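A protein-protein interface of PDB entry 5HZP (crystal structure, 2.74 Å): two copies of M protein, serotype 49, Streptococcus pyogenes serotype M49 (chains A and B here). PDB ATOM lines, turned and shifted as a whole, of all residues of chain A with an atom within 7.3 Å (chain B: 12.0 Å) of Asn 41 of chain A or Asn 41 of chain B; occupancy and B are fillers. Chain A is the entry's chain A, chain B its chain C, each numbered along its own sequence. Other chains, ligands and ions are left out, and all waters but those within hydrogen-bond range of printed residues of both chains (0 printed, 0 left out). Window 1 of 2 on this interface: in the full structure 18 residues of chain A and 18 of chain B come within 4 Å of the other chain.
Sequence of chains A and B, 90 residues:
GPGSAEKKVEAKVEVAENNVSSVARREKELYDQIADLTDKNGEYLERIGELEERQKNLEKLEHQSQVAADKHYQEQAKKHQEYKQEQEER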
ATOM      1  N   ASP A  36     -31.053 -23.720   8.391  1.00  0.00           N
ATOM      2  CA  ASP A  36     -30.016 -24.718   8.540  1.00  0.00           C
ATOM      3  C   ASP A  36     -28.631 -24.109   8.437  1.00  0.00           C
ATOM      4  O   ASP A  36     -27.767 -24.375   9.253  1.00  0.00           O
ATOM      5  CB  ASP A  36     -30.191 -25.807   7.505  1.00  0.00           C
ATOM      6  CG  ASP A  36     -31.322 -26.729   7.846  1.00  0.00           C
ATOM      7  OD1 ASP A  36     -31.858 -26.603   8.974  1.00  0.00           O
ATOM      8  OD2 ASP A  36     -31.677 -27.574   6.994  1.00  0.00           O
ATOM      9  N   LEU A  37     -28.424 -23.280   7.437  1.00  0.00           N
ATOM     10  CA  LEU A  37     -27.171 -22.581   7.330  1.00  0.00           C
ATOM     11  C   LEU A  37     -26.875 -21.781   8.599  1.00  0.00           C
ATOM     12  O   LEU A  37     -25.766 -21.826   9.096  1.00  0.00           O
ATOM     13  CB  LEU A  37     -27.181 -21.672   6.103  1.00  0.00           C
ATOM     14  CG  LEU A  37     -27.416 -22.419   4.791  1.00  0.00           C
ATOM     15  CD1 LEU A  37     -26.830 -21.650   3.610  1.00  0.00           C
ATOM     16  CD2 LEU A  37     -26.849 -23.846   4.874  1.00  0.00           C
ATOM     17  N   THR A  38     -27.848 -21.065   9.151  1.00  0.00           N
ATOM     18  CA  THR A  38     -27.541 -20.274  10.337  1.00  0.00           C
ATOM     19  C   THR A  38     -27.278 -21.214  11.509  1.00  0.00           C
ATOM     20  O   THR A  38     -26.736 -20.795  12.539  1.00  0.00           O
ATOM     21  CB  THR A  38     -28.669 -19.268  10.729  1.00  0.00           C
ATOM     22  OG1 THR A  38     -29.718 -19.962  11.409  1.00  0.00           O
ATOM     23  CG2 THR A  38     -29.222 -18.514   9.517  1.00  0.00           C
ATOM     24  N   ASP A  39     -27.652 -22.484  11.352  1.00  0.00           N
ATOM     25  CA  ASP A  39     -27.378 -23.498  12.383  1.00  0.00           C
ATOM     26  C   ASP A  39     -25.966 -24.106  12.259  1.00  0.00           C
ATOM     27  O   ASP A  39     -25.247 -24.208  13.252  1.00  0.00           O
ATOM     28  CB  ASP A  39     -28.422 -24.613  12.338  1.00  0.00           C
ATOM     29  CG  ASP A  39     -29.602 -24.340  13.248  1.00  0.00           C
ATOM     30  OD1 ASP A  39     -29.449 -23.531  14.190  1.00  0.00           O
ATOM     31  OD2 ASP A  39     -30.680 -24.934  13.029  1.00  0.00           O
ATOM     32  N   LYS A  40     -25.601 -24.528  11.048  1.00  0.00           N
ATOM     33  CA  LYS A  40     -24.237 -24.912  10.731  1.00  0.00           C
ATOM     34  C   LYS A  40     -23.326 -23.799  11.191  1.00  0.00           C
ATOM     35  O   LYS A  40     -22.479 -24.013  12.044  1.00  0.00           O
ATOM     36  CB  LYS A  40     -24.050 -25.175   9.230  1.00  0.00           C
ATOM     37  CG  LYS A  40     -24.713 -26.449   8.695  1.00  0.00           C
ATOM     38  CD  LYS A  40     -24.755 -27.580   9.728  1.00  0.00           C
ATOM     39  CE  LYS A  40     -23.385 -28.245   9.928  1.00  0.00           C
ATOM     40  NZ  LYS A  40     -23.508 -29.544  10.661  1.00  0.00           N
ATOM     41  N   ASN A  41     -23.525 -22.602  10.651  1.00  0.00           N
ATOM     42  CA  ASN A  41     -22.850 -21.404  11.142  1.00  0.00           C
ATOM     43  C   ASN A  41     -22.689 -21.357  12.655  1.00  0.00           C
ATOM     44  O   ASN A  41     -21.776 -20.743  13.161  1.00  0.00           O
ATOM     45  CB  ASN A  41     -23.607 -20.163  10.711  1.00  0.00           C
ATOM     46  CG  ASN A  41     -23.153 -19.642   9.383  1.00  0.00           C
ATOM     47  OD1 ASN A  41     -23.264 -18.450   9.132  1.00  0.00           O
ATOM     48  ND2 ASN A  41     -22.646 -20.522   8.514  1.00  0.00           N
ATOM     49  N   GLY A  42     -23.579 -22.003  13.385  1.00  0.00           N
ATOM     50  CA  GLY A  42     -23.492 -21.971  14.827  1.00  0.00           C
ATOM     51  C   GLY A  42     -22.573 -23.053  15.356  1.00  0.00           C
ATOM     52  O   GLY A  42     -21.770 -22.790  16.234  1.00  0.00           O
ATOM     53  N   GLU A  43     -22.706 -24.266  14.823  1.00  0.00           N
ATOM     54  CA  GLU A  43     -21.856 -25.387  15.195  1.00  0.00           C
ATOM     55  C   GLU A  43     -20.417 -25.092  14.817  1.00  0.00           C
ATOM     56  O   GLU A  43     -19.480 -25.601  15.435  1.00  0.00           O
ATOM     57  CB  GLU A  43     -22.300 -26.680  14.508  1.00  0.00           C
ATOM     58  CG  GLU A  43     -23.578 -27.290  15.049  1.00  0.00           C
ATOM     59  CD  GLU A  43     -24.105 -28.408  14.157  1.00  0.00           C
ATOM     60  OE1 GLU A  43     -23.272 -29.035  13.458  1.00  0.00           O
ATOM     61  OE2 GLU A  43     -25.344 -28.646  14.154  1.00  0.00           O
ATOM     62  N   TYR A  44     -20.234 -24.268  13.799  1.00  0.00           N
ATOM     63  CA  TYR A  44     -18.897 -24.067  13.310  1.00  0.00           C
ATOM     64  C   TYR A  44     -18.125 -23.165  14.248  1.00  0.00           C
ATOM     65  O   TYR A  44     -17.101 -23.596  14.774  1.00  0.00           O
ATOM     66  CB  TYR A  44     -18.913 -23.555  11.878  1.00  0.00           C
ATOM     67  CG  TYR A  44     -19.235 -24.692  10.942  1.00  0.00           C
ATOM     68  CD1 TYR A  44     -19.206 -26.003  11.392  1.00  0.00           C
ATOM     69  CD2 TYR A  44     -19.601 -24.465   9.624  1.00  0.00           C
ATOM     70  CE1 TYR A  44     -19.507 -27.061  10.552  1.00  0.00           C
ATOM     71  CE2 TYR A  44     -19.916 -25.519   8.772  1.00  0.00           C
ATOM     72  CZ  TYR A  44     -19.867 -26.812   9.242  1.00  0.00           C
ATOM     73  OH  TYR A  44     -20.175 -27.850   8.393  1.00  0.00           O
ATOM     74  N   LEU A  45     -18.599 -21.956  14.532  1.00  0.00           N
ATOM     75  CA  LEU A  45     -17.791 -21.125  15.428  1.00  0.00           C
ATOM     76  C   LEU A  45     -17.969 -21.541  16.895  1.00  0.00           C
ATOM     77  O   LEU A  45     -17.512 -20.866  17.821  1.00  0.00           O
ATOM     78  CB  LEU A  45     -18.097 -19.646  15.237  1.00  0.00           C
ATOM     79  CG  LEU A  45     -19.441 -19.356  14.616  1.00  0.00           C
ATOM     80  CD1 LEU A  45     -20.486 -19.529  15.694  1.00  0.00           C
ATOM     81  CD2 LEU A  45     -19.458 -17.961  14.050  1.00  0.00           C
ATOM     82  N   GLU A  46     -18.638 -22.667  17.092  1.00  0.00           N
ATOM     83  CA  GLU A  46     -18.643 -23.345  18.370  1.00  0.00           C
ATOM     84  C   GLU A  46     -17.306 -24.053  18.480  1.00  0.00           C
ATOM     85  O   GLU A  46     -16.703 -24.110  19.547  1.00  0.00           O
ATOM     86  CB  GLU A  46     -19.804 -24.334  18.444  1.00  0.00           C
ATOM     87  CG  GLU A  46     -19.716 -25.394  19.503  1.00  0.00           C
ATOM     88  CD  GLU A  46     -20.218 -24.898  20.830  1.00  0.00           C
ATOM     89  OE1 GLU A  46     -19.619 -23.930  21.348  1.00  0.00           O
ATOM     90  OE2 GLU A  46     -21.209 -25.467  21.348  1.00  0.00           O
ATOM     91  N   ASP B  32     -30.133 -14.221  -1.519  1.00  0.00           N
ATOM     92  CA  ASP B  32     -28.997 -13.513  -0.970  1.00  0.00           C
ATOM     93  C   ASP B  32     -28.546 -14.079   0.397  1.00  0.00           C
ATOM     94  O   ASP B  32     -27.354 -14.208   0.655  1.00  0.00           O
ATOM     95  CB  ASP B  32     -29.330 -12.027  -0.865  1.00  0.00           C
ATOM     96  CG  ASP B  32     -29.118 -11.309  -2.174  1.00  0.00           C
ATOM     97  OD1 ASP B  32     -28.843 -12.016  -3.167  1.00  0.00           O
ATOM     98  OD2 ASP B  32     -29.212 -10.059  -2.222  1.00  0.00           O
ATOM     99  N   GLN B  33     -29.485 -14.411   1.272  1.00  0.00           N
ATOM    100  CA  GLN B  33     -29.130 -15.070   2.512  1.00  0.00           C
ATOM    101  C   GLN B  33     -28.424 -16.378   2.189  1.00  0.00           C
ATOM    102  O   GLN B  33     -27.288 -16.575   2.589  1.00  0.00           O
ATOM    103  CB  GLN B  33     -30.359 -15.336   3.387  1.00  0.00           C
ATOM    104  CG  GLN B  33     -30.915 -14.126   4.119  1.00  0.00           C
ATOM    105  CD  GLN B  33     -32.115 -14.485   4.994  1.00  0.00           C
ATOM    106  OE1 GLN B  33     -31.997 -15.245   5.969  1.00  0.00           O
ATOM    107  NE2 GLN B  33     -33.285 -13.948   4.638  1.00  0.00           N
ATOM    108  N   ILE B  34     -29.083 -17.254   1.438  1.00  0.00           N
ATOM    109  CA  ILE B  34     -28.517 -18.553   1.082  1.00  0.00           C
ATOM    110  C   ILE B  34     -27.147 -18.402   0.409  1.00  0.00           C
ATOM    111  O   ILE B  34     -26.359 -19.326   0.390  1.00  0.00           O
ATOM    112  CB  ILE B  34     -29.477 -19.357   0.166  1.00  0.00           C
ATOM    113  CG1 ILE B  34     -30.719 -19.772   0.946  1.00  0.00           C
ATOM    114  CG2 ILE B  34     -28.842 -20.634  -0.378  1.00  0.00           C
ATOM    115  CD1 ILE B  34     -31.516 -20.833   0.252  1.00  0.00           C
ATOM    116  N   ALA B  35     -26.825 -17.234  -0.113  1.00  0.00           N
ATOM    117  CA  ALA B  35     -25.474 -17.059  -0.603  1.00  0.00           C
ATOM    118  C   ALA B  35     -24.555 -16.719   0.584  1.00  0.00           C
ATOM    119  O   ALA B  35     -23.701 -17.526   0.987  1.00  0.00           O
ATOM    120  CB  ALA B  35     -25.418 -15.984  -1.671  1.00  0.00           C
ATOM    121  N   ASP B  36     -24.788 -15.545   1.177  1.00  0.00           N
ATOM    122  CA  ASP B  36     -23.937 -14.977   2.227  1.00  0.00           C
ATOM    123  C   ASP B  36     -23.921 -15.828   3.493  1.00  0.00           C
ATOM    124  O   ASP B  36     -23.401 -15.413   4.527  1.00  0.00           O
ATOM    125  CB  ASP B  36     -24.390 -13.548   2.594  1.00  0.00           C
ATOM    126  CG  ASP B  36     -24.527 -12.606   1.365  1.00  0.00           C
ATOM    127  OD1 ASP B  36     -23.712 -12.689   0.416  1.00  0.00           O
ATOM    128  OD2 ASP B  36     -25.457 -11.762   1.362  1.00  0.00           O
ATOM    129  N   LEU B  37     -24.515 -17.008   3.409  1.00  0.00           N
ATOM    130  CA  LEU B  37     -24.522 -17.961   4.499  1.00  0.00           C
ATOM    131  C   LEU B  37     -23.680 -19.108   4.035  1.00  0.00           C
ATOM    132  O   LEU B  37     -22.701 -19.469   4.665  1.00  0.00           O
ATOM    133  CB  LEU B  37     -25.943 -18.428   4.827  1.00  0.00           C
ATOM    134  CG  LEU B  37     -26.477 -18.187   6.232  1.00  0.00           C
ATOM    135  CD1 LEU B  37     -25.863 -16.908   6.804  1.00  0.00           C
ATOM    136  CD2 LEU B  37     -28.001 -18.116   6.192  1.00  0.00           C
ATOM    137  N   THR B  38     -24.068 -19.662   2.895  1.00  0.00           N
ATOM    138  CA  THR B  38     -23.334 -20.736   2.253  1.00  0.00           C
ATOM    139  C   THR B  38     -21.842 -20.388   2.158  1.00  0.00           C
ATOM    140  O   THR B  38     -20.972 -21.246   2.277  1.00  0.00           O
ATOM    141  CB  THR B  38     -23.930 -21.013   0.850  1.00  0.00           C
ATOM    142  OG1 THR B  38     -24.872 -22.107   0.924  1.00  0.00           O
ATOM    143  CG2 THR B  38     -22.834 -21.284  -0.201  1.00  0.00           C
ATOM    144  N   ASP B  39     -21.562 -19.106   1.985  1.00  0.00           N
ATOM    145  CA  ASP B  39     -20.205 -18.642   1.821  1.00  0.00           C
ATOM    146  C   ASP B  39     -19.471 -18.556   3.151  1.00  0.00           C
ATOM    147  O   ASP B  39     -18.253 -18.801   3.223  1.00  0.00           O
ATOM    148  CB  ASP B  39     -20.189 -17.277   1.140  1.00  0.00           C
ATOM    149  CG  ASP B  39     -20.044 -17.377  -0.356  1.00  0.00           C
ATOM    150  OD1 ASP B  39     -20.534 -18.371  -0.946  1.00  0.00           O
ATOM    151  OD2 ASP B  39     -19.435 -16.454  -0.935  1.00  0.00           O
ATOM    152  N   LYS B  40     -20.185 -18.187   4.205  1.00  0.00           N
ATOM    153  CA  LYS B  40     -19.496 -18.040   5.469  1.00  0.00           C
ATOM    154  C   LYS B  40     -19.522 -19.384   6.195  1.00  0.00           C
ATOM    155  O   LYS B  40     -18.797 -19.581   7.162  1.00  0.00           O
ATOM    156  CB  LYS B  40     -20.092 -16.902   6.308  1.00  0.00           C
ATOM    157  CG  LYS B  40     -21.372 -17.232   7.042  1.00  0.00           C
ATOM    158  CD  LYS B  40     -21.677 -16.171   8.110  1.00  0.00           C
ATOM    159  CE  LYS B  40     -21.832 -14.766   7.542  1.00  0.00           C
ATOM    160  NZ  LYS B  40     -22.186 -13.775   8.611  1.00  0.00           N
ATOM    161  N   ASN B  41     -20.329 -20.316   5.705  1.00  0.00           N
ATOM    162  CA  ASN B  41     -20.193 -21.722   6.078  1.00  0.00           C
ATOM    163  C   ASN B  41     -18.833 -22.258   5.704  1.00  0.00           C
ATOM    164  O   ASN B  41     -18.231 -23.022   6.449  1.00  0.00           O
ATOM    165  CB  ASN B  41     -21.222 -22.589   5.376  1.00  0.00           C
ATOM    166  CG  ASN B  41     -22.022 -23.427   6.325  1.00  0.00           C
ATOM    167  OD1 ASN B  41     -22.512 -22.929   7.343  1.00  0.00           O
ATOM    168  ND2 ASN B  41     -22.181 -24.712   5.998  1.00  0.00           N
ATOM    169  N   GLY B  42     -18.366 -21.888   4.519  1.00  0.00           N
ATOM    170  CA  GLY B  42     -17.138 -22.450   4.006  1.00  0.00           C
ATOM    171  C   GLY B  42     -15.923 -21.649   4.434  1.00  0.00           C
ATOM    172  O   GLY B  42     -14.805 -21.946   4.022  1.00  0.00           O
ATOM    173  N   GLU B  43     -16.138 -20.613   5.238  1.00  0.00           N
ATOM    174  CA  GLU B  43     -15.030 -19.814   5.731  1.00  0.00           C
ATOM    175  C   GLU B  43     -14.829 -20.132   7.208  1.00  0.00           C
ATOM    176  O   GLU B  43     -13.836 -19.766   7.822  1.00  0.00           O
ATOM    177  CB  GLU B  43     -15.276 -18.320   5.523  1.00  0.00           C
ATOM    178  CG  GLU B  43     -15.838 -17.584   6.736  1.00  0.00           C
ATOM    179  CD  GLU B  43     -15.633 -16.069   6.650  1.00  0.00           C
ATOM    180  OE1 GLU B  43     -15.771 -15.508   5.536  1.00  0.00           O
ATOM    181  OE2 GLU B  43     -15.331 -15.437   7.692  1.00  0.00           O
ATOM    182  N   TYR B  44     -15.794 -20.826   7.772  1.00  0.00           N
ATOM    183  CA  TYR B  44     -15.699 -21.249   9.137  1.00  0.00           C
ATOM    184  C   TYR B  44     -15.007 -22.597   9.074  1.00  0.00           C
ATOM    185  O   TYR B  44     -14.165 -22.937   9.914  1.00  0.00           O
ATOM    186  CB  TYR B  44     -17.087 -21.304   9.779  1.00  0.00           C
ATOM    187  CG  TYR B  44     -17.695 -19.920  10.015  1.00  0.00           C
ATOM    188  CD1 TYR B  44     -16.918 -18.772   9.923  1.00  0.00           C
ATOM    189  CD2 TYR B  44     -19.038 -19.766  10.332  1.00  0.00           C
ATOM    190  CE1 TYR B  44     -17.464 -17.510  10.141  1.00  0.00           C
ATOM    191  CE2 TYR B  44     -19.595 -18.507  10.550  1.00  0.00           C
ATOM    192  CZ  TYR B  44     -18.801 -17.384  10.459  1.00  0.00           C
ATOM    193  OH  TYR B  44     -19.344 -16.132  10.677  1.00  0.00           O
ATOM    194  N   LEU B  45     -15.339 -23.340   8.029  1.00  0.00           N
ATOM    195  CA  LEU B  45     -14.603 -24.543   7.689  1.00  0.00           C
ATOM    196  C   LEU B  45     -13.133 -24.236   7.336  1.00  0.00           C
ATOM    197  O   LEU B  45     -12.223 -24.995   7.684  1.00  0.00           O
ATOM    198  CB  LEU B  45     -15.296 -25.252   6.528  1.00  0.00           C
ATOM    199  CG  LEU B  45     -15.955 -26.546   6.954  1.00  0.00           C
ATOM    200  CD1 LEU B  45     -16.522 -26.343   8.321  1.00  0.00           C
ATOM    201  CD2 LEU B  45     -17.051 -26.877   6.001  1.00  0.00           C
ATOM    202  N   GLU B  46     -12.914 -23.128   6.632  1.00  0.00           N
ATOM    203  CA  GLU B  46     -11.569 -22.696   6.285  1.00  0.00           C
ATOM    204  C   GLU B  46     -10.774 -22.488   7.571  1.00  0.00           C
ATOM    205  O   GLU B  46      -9.576 -22.724   7.614  1.00  0.00           O
ATOM    206  CB  GLU B  46     -11.606 -21.398   5.460  1.00  0.00           C
ATOM    207  CG  GLU B  46     -10.275 -20.920   4.867  1.00  0.00           C
ATOM    208  CD  GLU B  46     -10.112 -21.310   3.393  1.00  0.00           C
ATOM    209  OE1 GLU B  46      -9.537 -20.507   2.610  1.00  0.00           O
ATOM    210  OE2 GLU B  46     -10.561 -22.425   3.022  1.00  0.00           O
ATOM    211  N   ARG B  47     -11.462 -22.049   8.618  1.00  0.00           N
ATOM    212  CA  ARG B  47     -10.801 -21.645   9.836  1.00  0.00           C
ATOM    213  C   ARG B  47     -10.520 -22.878  10.678  1.00  0.00           C
ATOM    214  O   ARG B  47      -9.424 -23.035  11.216  1.00  0.00           O
ATOM    215  CB  ARG B  47     -11.655 -20.637  10.599  1.00  0.00           C
ATOM    216  CG  ARG B  47     -11.039 -20.159  11.895  1.00  0.00           C
ATOM    217  CD  ARG B  47     -10.406 -18.797  11.744  1.00  0.00           C
ATOM    218  NE  ARG B  47      -9.453 -18.541  12.818  1.00  0.00           N
ATOM    219  CZ  ARG B  47      -8.132 -18.688  12.708  1.00  0.00           C
ATOM    220  NH1 ARG B  47      -7.587 -19.081  11.554  1.00  0.00           N
ATOM    221  NH2 ARG B  47      -7.351 -18.423  13.752  1.00  0.00           N
ATOM    222  N   ILE B  48     -11.515 -23.751  10.783  1.00  0.00           N
ATOM    223  CA  ILE B  48     -11.364 -25.023  11.471  1.00  0.00           C
ATOM    224  C   ILE B  48     -10.230 -25.814  10.822  1.00  0.00           C
ATOM    225  O   ILE B  48      -9.449 -26.482  11.501  1.00  0.00           O
ATOM    226  CB  ILE B  48     -12.684 -25.817  11.450  1.00  0.00           C
ATOM    227  CG1 ILE B  48     -13.674 -25.224  12.456  1.00  0.00           C
ATOM    228  CG2 ILE B  48     -12.481 -27.288  11.751  1.00  0.00           C
ATOM    229  CD1 ILE B  48     -15.115 -25.643  12.214  1.00  0.00           C
ATOM    230  N   GLY B  49     -10.105 -25.701   9.508  1.00  0.00           N
ATOM    231  CA  GLY B  49      -8.969 -26.289   8.828  1.00  0.00           C
ATOM    232  C   GLY B  49      -7.645 -25.760   9.360  1.00  0.00           C
ATOM    233  O   GLY B  49      -6.872 -26.525   9.895  1.00  0.00           O
ATOM    234  N   GLU B  50      -7.409 -24.454   9.199  1.00  0.00           N
ATOM    235  CA  GLU B  50      -6.207 -23.771   9.661  1.00  0.00           C
ATOM    236  C   GLU B  50      -5.919 -24.120  11.107  1.00  0.00           C
ATOM    237  O   GLU B  50      -4.768 -24.257  11.492  1.00  0.00           O
ATOM    238  CB  GLU B  50      -6.332 -22.237   9.558  1.00  0.00           C
ATOM    239  CG  GLU B  50      -6.761 -21.671   8.230  1.00  0.00           C
ATOM    240  CD  GLU B  50      -5.648 -21.626   7.220  1.00  0.00           C
ATOM    241  OE1 GLU B  50      -5.958 -21.621   6.005  1.00  0.00           O
ATOM    242  OE2 GLU B  50      -4.470 -21.586   7.640  1.00  0.00           O
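The side-chain amide oxygen (OD1) of Asn 41 of chain B is in hydrogen-bond range of the side-chain amide nitrogen (ND2) of Asn 41 of chain A, 2.7 Å away.
The side-chain hydroxyl (OG1) of Thr 38 of chain B sits close to the backbone carbonyl oxygen (O) of Ile 34 of chain B, at 3.2 Å.
The side-chain amide nitrogen (ND2) of Asn 41 of chain A sits close to the backbone carbonyl oxygen (O) of Leu 37 of chain A, at 3.4 Å.
NZ of Lys 40 of chain A lies within salt-bridge range of OE1 of Glu 43 of chain A, at 2.9 Å.
Leu 37 of chain B touches Leu 37 of chain A (CB to CD1, 3.6 Å).
Leu 37 of chain A touches Asn 41 of chain B.
Asn 41 of chain B touches Lys 40 of chain A.
Leu 37 of chain B touches Asn 41 of chain A (CD1 to OD1, 3.8 Å).
Lys 40 of chain B touches Asn 41 of chain A.
CE2 of Tyr 44 of chain A touches ND2 of Asn 41 of chain B (3.7 Å).
Tyr 44 of chain B touches Tyr 44 of chain A.
Tyr 44 of chain A touches Leu 45 of chain B (CZ to CD1, 3.5 Å).
O of Tyr 44 of chain A touches CD1 of Ile 48 of chain B, at 3.8 Å.
Leu 45 of chain A touches Tyr 44 of chain B (CD2 to CE2, 3.5 Å).
Of chain B, only Leu 37 (3.8 Å), Lys 40 (3.0 Å), Asn 41 (2.7 Å) and Tyr 44 (3.9 Å) come within 4 Å of Asn 41 of chain A.
Of chain A, only Leu 37, Lys 40, Asn 41 and Tyr 44 come within 4 Å of Asn 41 of chain B.
No residue of chain B comes within 4 Å of Gly 42 of chain A.
No residue of chain B comes within 4 Å of Glu 43 of chain A.
Tyr 44 of chain A touches just these residues of chain B: Asn 41, Tyr 44, Leu 45 and Ile 48.
Leu 45 of chain A touches just one residue of chain B: Tyr 44.
Printed residues of chain B within 4 Å of Leu 37 of chain A: Ile 34 (3.999 Å), Leu 37 (3.6 Å), Thr 38 (3.4 Å) and Asn 41 (3.9 Å).
Of the printed residues of chain A, Thr 38 of chain B touches Leu 37.
Of the printed residues of chain A, Ile 34 of chain B touches Leu 37 (3.999 Å).
Printed residues of chain A within 4 Å of Tyr 44 of chain B: Asn 41 (3.9 Å), Tyr 44 (3.6 Å) and Leu 45 (3.5 Å).
The nearest printed residue of chain A that does not touch Leu 37 of chain B is Asp 36 of chain A (6.4 Å).
Of the 19 printed residues of chain B, 8 touch a printed residue of chain A.
Printed residues of chain B that touch a printed residue of chain A: Ile 34, Leu 37, Thr 38, Lys 40, Asn 41, Tyr 44, Leu 45 and Ile 48.
Of the 11 printed residues of chain A, 6 touch a printed residue of chain B.
Hydrophobic or aromatic side chains of chain A within 4 Å of the printed part of chain B: Leu 37, Tyr 44 and Leu 45.
Leu 37 of chain A touches its own counterpart, Leu 37 of chain B.
Lys 40 of chain A touches Asn 41 of chain B, and with the chains exchanged Asn 41 of chain A touches Lys 40 of chain B.
Asn 41 of chain B touches its own counterpart, Asn 41 of chain A.
Tyr 44 of chain B touches its own counterpart, Tyr 44 of chain A.
Positions printed for both chains: 36, 37, 38, 39, 40, 41, 42, 43, 44, 45 and 46.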
